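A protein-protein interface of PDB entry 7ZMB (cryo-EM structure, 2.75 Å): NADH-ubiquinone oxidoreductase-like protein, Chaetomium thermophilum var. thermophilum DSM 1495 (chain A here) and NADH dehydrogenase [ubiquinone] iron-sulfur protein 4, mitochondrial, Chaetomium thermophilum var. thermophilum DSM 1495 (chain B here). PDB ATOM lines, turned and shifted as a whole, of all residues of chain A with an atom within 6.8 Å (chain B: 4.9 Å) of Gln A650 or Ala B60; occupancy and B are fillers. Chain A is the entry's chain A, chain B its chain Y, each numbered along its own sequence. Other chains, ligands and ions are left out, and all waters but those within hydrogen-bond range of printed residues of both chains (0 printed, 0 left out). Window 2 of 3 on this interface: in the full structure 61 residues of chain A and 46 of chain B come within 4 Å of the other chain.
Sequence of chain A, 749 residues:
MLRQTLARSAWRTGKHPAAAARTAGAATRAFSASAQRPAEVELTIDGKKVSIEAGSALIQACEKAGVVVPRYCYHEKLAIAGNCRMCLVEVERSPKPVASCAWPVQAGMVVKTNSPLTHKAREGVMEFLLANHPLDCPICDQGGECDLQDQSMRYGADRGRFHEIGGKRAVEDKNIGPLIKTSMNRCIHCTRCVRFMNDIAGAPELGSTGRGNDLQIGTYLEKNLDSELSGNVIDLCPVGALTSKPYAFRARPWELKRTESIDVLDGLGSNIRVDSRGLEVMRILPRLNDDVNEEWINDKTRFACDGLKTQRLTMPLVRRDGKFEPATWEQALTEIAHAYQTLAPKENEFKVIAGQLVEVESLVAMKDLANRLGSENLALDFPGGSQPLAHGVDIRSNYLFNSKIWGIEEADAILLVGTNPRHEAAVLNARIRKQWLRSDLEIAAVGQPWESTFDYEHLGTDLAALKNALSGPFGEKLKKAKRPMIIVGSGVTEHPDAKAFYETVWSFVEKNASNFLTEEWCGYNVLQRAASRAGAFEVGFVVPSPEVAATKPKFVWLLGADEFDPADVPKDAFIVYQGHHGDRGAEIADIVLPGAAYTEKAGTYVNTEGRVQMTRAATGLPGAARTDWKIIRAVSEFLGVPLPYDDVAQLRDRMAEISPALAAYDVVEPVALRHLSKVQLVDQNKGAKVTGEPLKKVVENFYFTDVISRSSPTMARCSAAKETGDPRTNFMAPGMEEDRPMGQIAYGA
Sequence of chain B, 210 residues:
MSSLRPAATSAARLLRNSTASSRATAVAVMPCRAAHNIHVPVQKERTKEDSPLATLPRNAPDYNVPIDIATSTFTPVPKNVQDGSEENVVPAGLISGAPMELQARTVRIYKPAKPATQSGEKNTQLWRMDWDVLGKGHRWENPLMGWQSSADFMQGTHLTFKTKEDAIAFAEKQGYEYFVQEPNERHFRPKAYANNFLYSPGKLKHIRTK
Of chain B, only Arg B58, Asn B59, Ala B60 and Pro B61 come within 4 Å of Gln A650.
Ala B60 touches one residue of chain A.
Of the printed residues of chain A, Lys B79 touches Asp A647 (3.2 Å) and Ala A649 (3.6 Å).
Of the printed residues of chain B, Asp A647 touches Lys B79 (3.2 Å).
Of the printed residues of chain A, Arg B58 touches Gln A650.
Printed residues of chain B within 4 Å of Ala A649: Lys B79.
Printed residues of chain A within 4 Å of Asn B59: Gln A650 (3.2 Å).
The nearest residue of chain B that does not touch Gln A650 is Pro B57 (4.6 Å).
Along chain A the printed residues that touch a printed residue of chain B span positions 646 to 650.
Printed residues of chain B that touch a printed residue of chain A: Arg B58, Asn B59, Ala B60, Pro B61 and Lys B79.
Hydrophobic or aromatic side chains of chain B that line the printed part of chain A: Ala B60 and Pro B61.
Among the printed residues, Asp or Glu carboxylates within 4 Å of a Lys or Arg side-chain nitrogen of the other chain: Asp A647 with Lys B79.
The backbone NH (N) of Asp A647 is in hydrogen-bond range of the side-chain amide oxygen (OE1) of Gln A650, 3.1 Å away.
OD1 of Asp A647 lies within hydrogen-bond range of N of Ala A649 (2.9 Å).
NE2 of Gln A650 is in hydrogen-bond range of O of Asn B59 (3.2 Å).
The side-chain carboxylate (OD1) of Asp A647 lies within salt-bridge range of the side-chain amino group (NZ) of Lys B79 (3.9 Å).
Among the printed residues, merely in contact across the chains: Gln A650 with Ala B60, Gln A650 with Pro B61, Asp A646 with Pro B61, Gln A650 with Arg B58 and Ala A649 with Lys B79.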
ATOM      1  N   PRO A 644      35.670 -19.810  -4.674  1.00  0.00           N
ATOM      2  CA  PRO A 644      35.704 -18.721  -5.670  1.00  0.00           C
ATOM      3  C   PRO A 644      34.845 -17.515  -5.331  1.00  0.00           C
ATOM      4  O   PRO A 644      35.282 -16.371  -5.490  1.00  0.00           O
ATOM      5  CB  PRO A 644      35.213 -19.418  -6.949  1.00  0.00           C
ATOM      6  CG  PRO A 644      34.669 -20.741  -6.511  1.00  0.00           C
ATOM      7  CD  PRO A 644      35.402 -21.115  -5.291  1.00  0.00           C
ATOM      8  N   TYR A 645      33.629 -17.751  -4.872  1.00  0.00           N
ATOM      9  CA  TYR A 645      32.686 -16.685  -4.564  1.00  0.00           C
ATOM     10  C   TYR A 645      33.092 -15.858  -3.346  1.00  0.00           C
ATOM     11  O   TYR A 645      33.679 -16.367  -2.388  1.00  0.00           O
ATOM     12  CB  TYR A 645      31.309 -17.317  -4.385  1.00  0.00           C
ATOM     13  CG  TYR A 645      31.276 -18.286  -3.247  1.00  0.00           C
ATOM     14  CD1 TYR A 645      31.032 -17.874  -1.953  1.00  0.00           C
ATOM     15  CD2 TYR A 645      31.570 -19.622  -3.468  1.00  0.00           C
ATOM     16  CE1 TYR A 645      31.039 -18.768  -0.919  1.00  0.00           C
ATOM     17  CE2 TYR A 645      31.577 -20.520  -2.445  1.00  0.00           C
ATOM     18  CZ  TYR A 645      31.312 -20.085  -1.169  1.00  0.00           C
ATOM     19  OH  TYR A 645      31.320 -20.974  -0.131  1.00  0.00           O
ATOM     20  N   ASP A 646      32.786 -14.557  -3.404  1.00  0.00           N
ATOM     21  CA  ASP A 646      32.998 -13.630  -2.294  1.00  0.00           C
ATOM     22  C   ASP A 646      31.726 -12.888  -1.913  1.00  0.00           C
ATOM     23  O   ASP A 646      31.789 -11.917  -1.153  1.00  0.00           O
ATOM     24  CB  ASP A 646      34.089 -12.609  -2.631  1.00  0.00           C
ATOM     25  CG  ASP A 646      35.457 -13.235  -2.792  1.00  0.00           C
ATOM     26  OD1 ASP A 646      35.685 -14.340  -2.263  1.00  0.00           O
ATOM     27  OD2 ASP A 646      36.314 -12.612  -3.446  1.00  0.00           O
ATOM     28  N   ASP A 647      30.574 -13.313  -2.422  1.00  0.00           N
ATOM     29  CA  ASP A 647      29.328 -12.588  -2.243  1.00  0.00           C
ATOM     30  C   ASP A 647      28.188 -13.584  -2.349  1.00  0.00           C
ATOM     31  O   ASP A 647      28.361 -14.697  -2.852  1.00  0.00           O
ATOM     32  CB  ASP A 647      29.189 -11.466  -3.281  1.00  0.00           C
ATOM     33  CG  ASP A 647      27.985 -10.577  -3.035  1.00  0.00           C
ATOM     34  OD1 ASP A 647      26.843 -11.069  -3.154  1.00  0.00           O
ATOM     35  OD2 ASP A 647      28.178  -9.384  -2.722  1.00  0.00           O
ATOM     36  N   VAL A 648      27.014 -13.181  -1.862  1.00  0.00           N
ATOM     37  CA  VAL A 648      25.892 -14.107  -1.827  1.00  0.00           C
ATOM     38  C   VAL A 648      25.394 -14.418  -3.232  1.00  0.00           C
ATOM     39  O   VAL A 648      24.917 -15.527  -3.492  1.00  0.00           O
ATOM     40  CB  VAL A 648      24.760 -13.567  -0.933  1.00  0.00           C
ATOM     41  CG1 VAL A 648      24.076 -12.384  -1.580  1.00  0.00           C
ATOM     42  CG2 VAL A 648      23.769 -14.670  -0.604  1.00  0.00           C
ATOM     43  N   ALA A 649      25.476 -13.458  -4.153  1.00  0.00           N
ATOM     44  CA  ALA A 649      25.043 -13.709  -5.520  1.00  0.00           C
ATOM     45  C   ALA A 649      25.944 -14.723  -6.206  1.00  0.00           C
ATOM     46  O   ALA A 649      25.459 -15.609  -6.919  1.00  0.00           O
ATOM     47  CB  ALA A 649      25.008 -12.404  -6.305  1.00  0.00           C
ATOM     48  N   GLN A 650      27.256 -14.620  -5.991  1.00  0.00           N
ATOM     49  CA  GLN A 650      28.177 -15.581  -6.581  1.00  0.00           C
ATOM     50  C   GLN A 650      27.937 -16.987  -6.052  1.00  0.00           C
ATOM     51  O   GLN A 650      28.101 -17.963  -6.788  1.00  0.00           O
ATOM     52  CB  GLN A 650      29.619 -15.174  -6.310  1.00  0.00           C
ATOM     53  CG  GLN A 650      30.165 -14.057  -7.129  1.00  0.00           C
ATOM     54  CD  GLN A 650      31.357 -13.419  -6.465  1.00  0.00           C
ATOM     55  OE1 GLN A 650      31.644 -13.676  -5.300  1.00  0.00           O
ATOM     56  NE2 GLN A 650      32.106 -12.644  -7.226  1.00  0.00           N
ATOM     57  N   LEU A 651      27.585 -17.109  -4.775  1.00  0.00           N
ATOM     58  CA  LEU A 651      27.246 -18.406  -4.216  1.00  0.00           C
ATOM     59  C   LEU A 651      25.872 -18.874  -4.670  1.00  0.00           C
ATOM     60  O   LEU A 651      25.660 -20.079  -4.845  1.00  0.00           O
ATOM     61  CB  LEU A 651      27.328 -18.345  -2.693  1.00  0.00           C
ATOM     62  CG  LEU A 651      26.692 -19.437  -1.838  1.00  0.00           C
ATOM     63  CD1 LEU A 651      27.275 -20.811  -2.141  1.00  0.00           C
ATOM     64  CD2 LEU A 651      26.855 -19.089  -0.382  1.00  0.00           C
ATOM     65  N   ARG A 652      24.932 -17.956  -4.880  1.00  0.00           N
ATOM     66  CA  ARG A 652      23.645 -18.372  -5.416  1.00  0.00           C
ATOM     67  C   ARG A 652      23.714 -18.692  -6.899  1.00  0.00           C
ATOM     68  O   ARG A 652      22.817 -19.369  -7.409  1.00  0.00           O
ATOM     69  CB  ARG A 652      22.581 -17.311  -5.139  1.00  0.00           C
ATOM     70  CG  ARG A 652      21.958 -17.484  -3.772  1.00  0.00           C
ATOM     71  CD  ARG A 652      21.177 -16.281  -3.340  1.00  0.00           C
ATOM     72  NE  ARG A 652      20.642 -16.482  -2.004  1.00  0.00           N
ATOM     73  CZ  ARG A 652      20.360 -15.499  -1.161  1.00  0.00           C
ATOM     74  NH1 ARG A 652      19.879 -15.780   0.039  1.00  0.00           N
ATOM     75  NH2 ARG A 652      20.565 -14.246  -1.525  1.00  0.00           N
ATOM     76  N   ASP A 653      24.745 -18.216  -7.603  1.00  0.00           N
ATOM     77  CA  ASP A 653      25.031 -18.744  -8.931  1.00  0.00           C
ATOM     78  C   ASP A 653      25.594 -20.158  -8.854  1.00  0.00           C
ATOM     79  O   ASP A 653      25.196 -21.030  -9.634  1.00  0.00           O
ATOM     80  CB  ASP A 653      25.990 -17.821  -9.677  1.00  0.00           C
ATOM     81  CG  ASP A 653      25.443 -16.419  -9.843  1.00  0.00           C
ATOM     82  OD1 ASP A 653      24.250 -16.280 -10.188  1.00  0.00           O
ATOM     83  OD2 ASP A 653      26.213 -15.453  -9.650  1.00  0.00           O
ATOM     84  N   ARG A 654      26.526 -20.405  -7.929  1.00  0.00           N
ATOM     85  CA  ARG A 654      26.938 -21.776  -7.640  1.00  0.00           C
ATOM     86  C   ARG A 654      25.761 -22.660  -7.281  1.00  0.00           C
ATOM     87  O   ARG A 654      25.678 -23.805  -7.733  1.00  0.00           O
ATOM     88  CB  ARG A 654      27.987 -21.807  -6.525  1.00  0.00           C
ATOM     89  CG  ARG A 654      28.416 -23.222  -6.198  1.00  0.00           C
ATOM     90  CD  ARG A 654      29.141 -23.927  -7.296  1.00  0.00           C
ATOM     91  NE  ARG A 654      29.531 -25.264  -6.862  1.00  0.00           N
ATOM     92  CZ  ARG A 654      30.035 -26.200  -7.657  1.00  0.00           C
ATOM     93  NH1 ARG A 654      30.203 -25.966  -8.943  1.00  0.00           N
ATOM     94  NH2 ARG A 654      30.346 -27.387  -7.163  1.00  0.00           N
ATOM     95  N   MET A 655      24.849 -22.152  -6.460  1.00  0.00           N
ATOM     96  CA  MET A 655      23.719 -22.956  -6.020  1.00  0.00           C
ATOM     97  C   MET A 655      22.867 -23.381  -7.206  1.00  0.00           C
ATOM     98  O   MET A 655      22.473 -24.546  -7.319  1.00  0.00           O
ATOM     99  CB  MET A 655      22.900 -22.158  -5.011  1.00  0.00           C
ATOM    100  CG  MET A 655      23.372 -22.304  -3.591  1.00  0.00           C
ATOM    101  SD  MET A 655      22.602 -21.085  -2.518  1.00  0.00           S
ATOM    102  CE  MET A 655      20.960 -21.764  -2.375  1.00  0.00           C
ATOM    103  N   PRO B  57      33.160  -9.624 -13.464  1.00  0.00           N
ATOM    104  CA  PRO B  57      33.278 -11.071 -13.652  1.00  0.00           C
ATOM    105  C   PRO B  57      32.237 -11.857 -12.860  1.00  0.00           C
ATOM    106  O   PRO B  57      32.534 -12.337 -11.767  1.00  0.00           O
ATOM    107  CB  PRO B  57      34.688 -11.369 -13.144  1.00  0.00           C
ATOM    108  CG  PRO B  57      35.457 -10.105 -13.407  1.00  0.00           C
ATOM    109  CD  PRO B  57      34.473  -8.959 -13.500  1.00  0.00           C
ATOM    110  N   ARG B  58      31.032 -11.976 -13.422  1.00  0.00           N
ATOM    111  CA  ARG B  58      29.938 -12.740 -12.825  1.00  0.00           C
ATOM    112  C   ARG B  58      29.585 -12.205 -11.434  1.00  0.00           C
ATOM    113  O   ARG B  58      29.713 -12.894 -10.419  1.00  0.00           O
ATOM    114  CB  ARG B  58      30.281 -14.233 -12.776  1.00  0.00           C
ATOM    115  CG  ARG B  58      29.079 -15.151 -12.643  1.00  0.00           C
ATOM    116  CD  ARG B  58      28.129 -14.997 -13.818  1.00  0.00           C
ATOM    117  NE  ARG B  58      27.061 -15.992 -13.784  1.00  0.00           N
ATOM    118  CZ  ARG B  58      25.929 -15.898 -14.472  1.00  0.00           C
ATOM    119  NH1 ARG B  58      25.711 -14.852 -15.255  1.00  0.00           N
ATOM    120  NH2 ARG B  58      25.013 -16.853 -14.377  1.00  0.00           N
ATOM    121  N   ASN B  59      29.143 -10.946 -11.410  1.00  0.00           N
ATOM    122  CA  ASN B  59      28.659 -10.290 -10.194  1.00  0.00           C
ATOM    123  C   ASN B  59      29.724 -10.307  -9.095  1.00  0.00           C
ATOM    124  O   ASN B  59      29.561 -10.919  -8.038  1.00  0.00           O
ATOM    125  CB  ASN B  59      27.355 -10.934  -9.713  1.00  0.00           C
ATOM    126  CG  ASN B  59      26.185 -10.631 -10.625  1.00  0.00           C
ATOM    127  OD1 ASN B  59      25.981  -9.487 -11.031  1.00  0.00           O
ATOM    128  ND2 ASN B  59      25.410 -11.656 -10.955  1.00  0.00           N
ATOM    129  N   ALA B  60      30.827  -9.618  -9.366  1.00  0.00           N
ATOM    130  CA  ALA B  60      31.868  -9.761  -8.358  1.00  0.00           C
ATOM    131  C   ALA B  60      31.924  -8.534  -7.451  1.00  0.00           C
ATOM    132  O   ALA B  60      31.669  -7.416  -7.905  1.00  0.00           O
ATOM    133  CB  ALA B  60      33.229  -9.967  -9.015  1.00  0.00           C
ATOM    134  N   PRO B  61      32.248  -8.721  -6.174  1.00  0.00           N
ATOM    135  CA  PRO B  61      32.577  -7.565  -5.330  1.00  0.00           C
ATOM    136  C   PRO B  61      33.774  -6.827  -5.904  1.00  0.00           C
ATOM    137  O   PRO B  61      34.869  -7.377  -6.013  1.00  0.00           O
ATOM    138  CB  PRO B  61      32.892  -8.196  -3.967  1.00  0.00           C
ATOM    139  CG  PRO B  61      33.152  -9.630  -4.250  1.00  0.00           C
ATOM    140  CD  PRO B  61      32.312  -9.987  -5.428  1.00  0.00           C
ATOM    141  N   ASP B  62      33.547  -5.580  -6.307  1.00  0.00           N
ATOM    142  CA  ASP B  62      34.614  -4.734  -6.827  1.00  0.00           C
ATOM    143  C   ASP B  62      35.236  -3.988  -5.656  1.00  0.00           C
ATOM    144  O   ASP B  62      34.603  -3.119  -5.055  1.00  0.00           O
ATOM    145  CB  ASP B  62      34.087  -3.768  -7.884  1.00  0.00           C
ATOM    146  CG  ASP B  62      35.199  -3.143  -8.701  1.00  0.00           C
ATOM    147  OD1 ASP B  62      35.771  -3.844  -9.561  1.00  0.00           O
ATOM    148  OD2 ASP B  62      35.512  -1.954  -8.477  1.00  0.00           O
ATOM    149  N   PRO B  78      30.360  -3.003  -3.165  1.00  0.00           N
ATOM    150  CA  PRO B  78      29.426  -3.037  -4.291  1.00  0.00           C
ATOM    151  C   PRO B  78      29.901  -3.934  -5.422  1.00  0.00           C
ATOM    152  O   PRO B  78      31.087  -4.000  -5.750  1.00  0.00           O
ATOM    153  CB  PRO B  78      29.381  -1.571  -4.740  1.00  0.00           C
ATOM    154  CG  PRO B  78      30.590  -0.918  -4.121  1.00  0.00           C
ATOM    155  CD  PRO B  78      31.329  -1.910  -3.296  1.00  0.00           C
ATOM    156  N   LYS B  79      28.950  -4.643  -6.026  1.00  0.00           N
ATOM    157  CA  LYS B  79      29.282  -5.419  -7.214  1.00  0.00           C
ATOM    158  C   LYS B  79      29.485  -4.510  -8.414  1.00  0.00           C
ATOM    159  O   LYS B  79      30.430  -4.694  -9.188  1.00  0.00           O
ATOM    160  CB  LYS B  79      28.201  -6.457  -7.497  1.00  0.00           C
ATOM    161  CG  LYS B  79      27.926  -7.392  -6.338  1.00  0.00           C
ATOM    162  CD  LYS B  79      27.018  -8.529  -6.765  1.00  0.00           C
ATOM    163  CE  LYS B  79      26.215  -9.059  -5.593  1.00  0.00           C
ATOM    164  NZ  LYS B  79      25.205  -8.068  -5.125  1.00  0.00           N
